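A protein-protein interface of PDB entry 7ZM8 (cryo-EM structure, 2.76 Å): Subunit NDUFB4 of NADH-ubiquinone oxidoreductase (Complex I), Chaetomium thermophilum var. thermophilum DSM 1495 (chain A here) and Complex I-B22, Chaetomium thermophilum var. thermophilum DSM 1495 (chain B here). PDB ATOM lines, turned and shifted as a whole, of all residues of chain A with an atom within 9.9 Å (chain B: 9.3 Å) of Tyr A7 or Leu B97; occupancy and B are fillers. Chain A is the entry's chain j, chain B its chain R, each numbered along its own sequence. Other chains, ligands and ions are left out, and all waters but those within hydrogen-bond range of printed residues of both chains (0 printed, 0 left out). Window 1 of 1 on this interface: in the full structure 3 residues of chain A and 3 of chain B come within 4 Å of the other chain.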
ATOM      1  N   LEU A   4      -2.168  -4.648  16.254  1.00  0.00           N
ATOM      2  CA  LEU A   4      -2.025  -5.689  17.309  1.00  0.00           C
ATOM      3  C   LEU A   4      -1.212  -5.130  18.470  1.00  0.00           C
ATOM      4  O   LEU A   4      -0.297  -4.337  18.222  1.00  0.00           O
ATOM      5  CB  LEU A   4      -1.304  -6.938  16.787  1.00  0.00           C
ATOM      6  CG  LEU A   4      -2.043  -7.810  15.782  1.00  0.00           C
ATOM      7  CD1 LEU A   4      -3.467  -8.084  16.235  1.00  0.00           C
ATOM      8  CD2 LEU A   4      -2.027  -7.135  14.433  1.00  0.00           C
ATOM      9  N   GLN A   5      -1.549  -5.531  19.687  1.00  0.00           N
ATOM     10  CA  GLN A   5      -0.717  -5.122  20.842  1.00  0.00           C
ATOM     11  C   GLN A   5       0.640  -5.795  20.699  1.00  0.00           C
ATOM     12  O   GLN A   5       0.694  -6.977  20.334  1.00  0.00           O
ATOM     13  CB  GLN A   5      -1.358  -5.496  22.179  1.00  0.00           C
ATOM     14  CG  GLN A   5      -1.827  -6.940  22.267  1.00  0.00           C
ATOM     15  CD  GLN A   5      -2.149  -7.308  23.692  1.00  0.00           C
ATOM     16  OE1 GLN A   5      -1.582  -6.760  24.635  1.00  0.00           O
ATOM     17  NE2 GLN A   5      -3.064  -8.247  23.861  1.00  0.00           N
ATOM     18  N   HIS A   6       1.688  -5.045  20.985  1.00  0.00           N
ATOM     19  CA  HIS A   6       3.054  -5.588  20.895  1.00  0.00           C
ATOM     20  C   HIS A   6       3.478  -5.888  22.331  1.00  0.00           C
ATOM     21  O   HIS A   6       2.696  -5.584  23.236  1.00  0.00           O
ATOM     22  CB  HIS A   6       3.912  -4.574  20.139  1.00  0.00           C
ATOM     23  CG  HIS A   6       3.975  -3.224  20.765  1.00  0.00           C
ATOM     24  ND1 HIS A   6       5.052  -2.811  21.513  1.00  0.00           N
ATOM     25  CD2 HIS A   6       3.107  -2.194  20.753  1.00  0.00           C
ATOM     26  CE1 HIS A   6       4.844  -1.588  21.944  1.00  0.00           C
ATOM     27  NE2 HIS A   6       3.660  -1.186  21.493  1.00  0.00           N
ATOM     28  N   TYR A   7       4.643  -6.492  22.515  1.00  0.00           N
ATOM     29  CA  TYR A   7       5.160  -6.759  23.866  1.00  0.00           C
ATOM     30  C   TYR A   7       5.700  -5.440  24.419  1.00  0.00           C
ATOM     31  O   TYR A   7       5.853  -4.497  23.654  1.00  0.00           O
ATOM     32  CB  TYR A   7       6.247  -7.823  23.794  1.00  0.00           C
ATOM     33  CG  TYR A   7       5.814  -9.244  23.546  1.00  0.00           C
ATOM     34  CD1 TYR A   7       5.053  -9.924  24.475  1.00  0.00           C
ATOM     35  CD2 TYR A   7       6.224  -9.935  22.420  1.00  0.00           C
ATOM     36  CE1 TYR A   7       4.668 -11.236  24.271  1.00  0.00           C
ATOM     37  CE2 TYR A   7       5.861 -11.252  22.207  1.00  0.00           C
ATOM     38  CZ  TYR A   7       5.073 -11.905  23.134  1.00  0.00           C
ATOM     39  OH  TYR A   7       4.681 -13.198  22.951  1.00  0.00           O
ATOM     40  N   LYS A   8       5.994  -5.392  25.719  1.00  0.00           N
ATOM     41  CA  LYS A   8       6.486  -4.148  26.355  1.00  0.00           C
ATOM     42  C   LYS A   8       7.961  -3.905  26.050  1.00  0.00           C
ATOM     43  O   LYS A   8       8.766  -4.803  26.275  1.00  0.00           O
ATOM     44  CB  LYS A   8       6.216  -4.196  27.857  1.00  0.00           C
ATOM     45  CG  LYS A   8       4.747  -4.243  28.249  1.00  0.00           C
ATOM     46  CD  LYS A   8       4.540  -4.332  29.745  1.00  0.00           C
ATOM     47  CE  LYS A   8       3.085  -4.502  30.130  1.00  0.00           C
ATOM     48  NZ  LYS A   8       2.507  -5.731  29.539  1.00  0.00           N
ATOM     49  N   ILE A   9       8.277  -2.707  25.561  1.00  0.00           N
ATOM     50  CA  ILE A   9       9.673  -2.311  25.224  1.00  0.00           C
ATOM     51  C   ILE A   9       9.976  -1.080  26.066  1.00  0.00           C
ATOM     52  O   ILE A   9       9.103  -0.220  26.175  1.00  0.00           O
ATOM     53  CB  ILE A   9       9.820  -2.007  23.718  1.00  0.00           C
ATOM     54  CG1 ILE A   9       9.066  -3.012  22.848  1.00  0.00           C
ATOM     55  CG2 ILE A   9      11.284  -1.916  23.318  1.00  0.00           C
ATOM     56  CD1 ILE A   9       9.693  -4.375  22.847  1.00  0.00           C
ATOM     57  N   ALA A  10      11.156  -1.030  26.666  1.00  0.00           N
ATOM     58  CA  ALA A  10      11.561   0.148  27.453  1.00  0.00           C
ATOM     59  C   ALA A  10      12.043   1.164  26.438  1.00  0.00           C
ATOM     60  O   ALA A  10      13.243   1.192  26.162  1.00  0.00           O
ATOM     61  CB  ALA A  10      12.665  -0.238  28.386  1.00  0.00           C
ATOM     62  N   MET A  11      11.108   1.940  25.892  1.00  0.00           N
ATOM     63  CA  MET A  11      11.465   2.869  24.801  1.00  0.00           C
ATOM     64  C   MET A  11      12.317   3.970  25.388  1.00  0.00           C
ATOM     65  O   MET A  11      11.853   4.666  26.298  1.00  0.00           O
ATOM     66  CB  MET A  11      10.198   3.471  24.214  1.00  0.00           C
ATOM     67  CG  MET A  11       9.590   2.585  23.151  1.00  0.00           C
ATOM     68  SD  MET A  11      10.697   2.484  21.727  1.00  0.00           S
ATOM     69  CE  MET A  11      10.415   0.799  21.199  1.00  0.00           C
ATOM     70  N   GLU B  92      11.705 -15.481  32.399  1.00  0.00           N
ATOM     71  CA  GLU B  92      10.274 -15.682  32.527  1.00  0.00           C
ATOM     72  C   GLU B  92       9.645 -15.945  31.163  1.00  0.00           C
ATOM     73  O   GLU B  92      10.087 -15.399  30.149  1.00  0.00           O
ATOM     74  CB  GLU B  92       9.624 -14.467  33.168  1.00  0.00           C
ATOM     75  CG  GLU B  92      10.042 -14.238  34.608  1.00  0.00           C
ATOM     76  CD  GLU B  92       9.555 -15.334  35.536  1.00  0.00           C
ATOM     77  OE1 GLU B  92       8.475 -15.902  35.275  1.00  0.00           O
ATOM     78  OE2 GLU B  92      10.256 -15.629  36.526  1.00  0.00           O
ATOM     79  N   PRO B  93       8.631 -16.861  31.142  1.00  0.00           N
ATOM     80  CA  PRO B  93       7.983 -17.264  29.915  1.00  0.00           C
ATOM     81  C   PRO B  93       7.404 -16.010  29.265  1.00  0.00           C
ATOM     82  O   PRO B  93       7.176 -15.043  29.956  1.00  0.00           O
ATOM     83  CB  PRO B  93       6.893 -18.207  30.411  1.00  0.00           C
ATOM     84  CG  PRO B  93       7.524 -18.889  31.559  1.00  0.00           C
ATOM     85  CD  PRO B  93       8.085 -17.684  32.263  1.00  0.00           C
ATOM     86  N   PRO B  94       7.159 -15.988  27.942  1.00  0.00           N
ATOM     87  CA  PRO B  94       6.676 -14.776  27.315  1.00  0.00           C
ATOM     88  C   PRO B  94       5.257 -14.476  27.828  1.00  0.00           C
ATOM     89  O   PRO B  94       4.553 -15.397  28.151  1.00  0.00           O
ATOM     90  CB  PRO B  94       6.768 -15.114  25.819  1.00  0.00           C
ATOM     91  CG  PRO B  94       7.647 -16.328  25.744  1.00  0.00           C
ATOM     92  CD  PRO B  94       7.325 -17.090  27.008  1.00  0.00           C
ATOM     93  N   PRO B  95       4.830 -13.206  27.954  1.00  0.00           N
ATOM     94  CA  PRO B  95       3.448 -12.903  28.333  1.00  0.00           C
ATOM     95  C   PRO B  95       2.531 -13.422  27.219  1.00  0.00           C
ATOM     96  O   PRO B  95       2.967 -13.490  26.096  1.00  0.00           O
ATOM     97  CB  PRO B  95       3.381 -11.383  28.446  1.00  0.00           C
ATOM     98  CG  PRO B  95       4.657 -10.879  27.806  1.00  0.00           C
ATOM     99  CD  PRO B  95       5.657 -12.015  27.838  1.00  0.00           C
ATOM    100  N   PRO B  96       1.257 -13.773  27.477  1.00  0.00           N
ATOM    101  CA  PRO B  96       0.445 -14.440  26.452  1.00  0.00           C
ATOM    102  C   PRO B  96      -0.196 -13.593  25.343  1.00  0.00           C
ATOM    103  O   PRO B  96      -1.376 -13.359  25.403  1.00  0.00           O
ATOM    104  CB  PRO B  96      -0.626 -15.096  27.326  1.00  0.00           C
ATOM    105  CG  PRO B  96      -0.808 -14.156  28.497  1.00  0.00           C
ATOM    106  CD  PRO B  96       0.566 -13.578  28.749  1.00  0.00           C
ATOM    107  N   LEU B  97       0.578 -13.228  24.320  1.00  0.00           N
ATOM    108  CA  LEU B  97       0.080 -12.354  23.226  1.00  0.00           C
ATOM    109  C   LEU B  97       0.125 -13.110  21.889  1.00  0.00           C
ATOM    110  O   LEU B  97       1.059 -13.894  21.707  1.00  0.00           O
ATOM    111  CB  LEU B  97       0.920 -11.072  23.172  1.00  0.00           C
ATOM    112  CG  LEU B  97       1.037 -10.253  24.455  1.00  0.00           C
ATOM    113  CD1 LEU B  97       1.679  -8.912  24.153  1.00  0.00           C
ATOM    114  CD2 LEU B  97      -0.320 -10.054  25.112  1.00  0.00           C
ATOM    115  N   LYS B  98      -0.798 -12.851  20.958  1.00  0.00           N
ATOM    116  CA  LYS B  98      -0.859 -13.654  19.706  1.00  0.00           C
ATOM    117  C   LYS B  98      -0.506 -12.832  18.466  1.00  0.00           C
ATOM    118  O   LYS B  98      -1.081 -11.758  18.279  1.00  0.00           O
ATOM    119  CB  LYS B  98      -2.300 -14.138  19.528  1.00  0.00           C
ATOM    120  CG  LYS B  98      -2.701 -15.338  20.376  1.00  0.00           C
ATOM    121  CD  LYS B  98      -2.023 -16.618  19.943  1.00  0.00           C
ATOM    122  CE  LYS B  98      -2.332 -16.990  18.507  1.00  0.00           C
ATOM    123  NZ  LYS B  98      -3.783 -17.195  18.293  1.00  0.00           N
ATOM    124  N   PHE B  99       0.397 -13.356  17.636  1.00  0.00           N
ATOM    125  CA  PHE B  99       0.916 -12.581  16.476  1.00  0.00           C
ATOM    126  C   PHE B  99       0.591 -13.272  15.150  1.00  0.00           C
ATOM    127  O   PHE B  99       0.440 -12.510  14.165  1.00  0.00           O
ATOM    128  CB  PHE B  99       2.426 -12.364  16.639  1.00  0.00           C
ATOM    129  CG  PHE B  99       2.716 -11.445  17.792  1.00  0.00           C
ATOM    130  CD1 PHE B  99       2.386 -10.103  17.717  1.00  0.00           C
ATOM    131  CD2 PHE B  99       3.241 -11.931  18.977  1.00  0.00           C
ATOM    132  CE1 PHE B  99       2.615  -9.261  18.791  1.00  0.00           C
ATOM    133  CE2 PHE B  99       3.464 -11.083  20.047  1.00  0.00           C
ATOM    134  CZ  PHE B  99       3.161  -9.749  19.951  1.00  0.00           C
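Of chain B, only Pro B95, Leu B97 and Phe B99 come within 4 Å of Tyr A7.
Leu B97 touches just these residues of chain A: Gln A5, His A6 and Tyr A7.
Of chain B, only Leu B97 (3.6 Å) comes within 4 Å of His A6.
Pro B95 touches one residue of chain A.
Of the printed residues of chain A, Phe B99 touches Gln A5 and Tyr A7.
Printed residues of chain B within 4 Å of Gln A5: Leu B97 (3.5 Å) and Phe B99 (3.4 Å).
Met A11 touches none of the printed residues of chain B.
The nearest residue of chain B that does not touch Tyr A7 is Pro B94 (4.03 Å).
CD2 of Leu B97 touches NE2 of Gln A5, at 3.5 Å.
Phe B99 touches Gln A5 (CE1 to O, 3.4 Å).
His A6 touches Leu B97 (O to CD1, 3.6 Å).
CE1 of Tyr A7 touches O of Pro B95 (3.4 Å).
Tyr A7 touches Leu B97 (CD1 to CD1, 3.5 Å).
CE2 of Tyr A7 touches CE2 of Phe B99, at 3.2 Å.
Hydrophobic or aromatic side chains of chain B that line the printed part of chain A: Pro B95, Leu B97 and Phe B99.
Of the 8 printed residues of chain A, 3 touch a printed residue of chain B.
Hydrophobic or aromatic side chains of chain A that line the printed part of chain B: Tyr A7.
Among the printed residues, 6 pairs touch across the chains.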
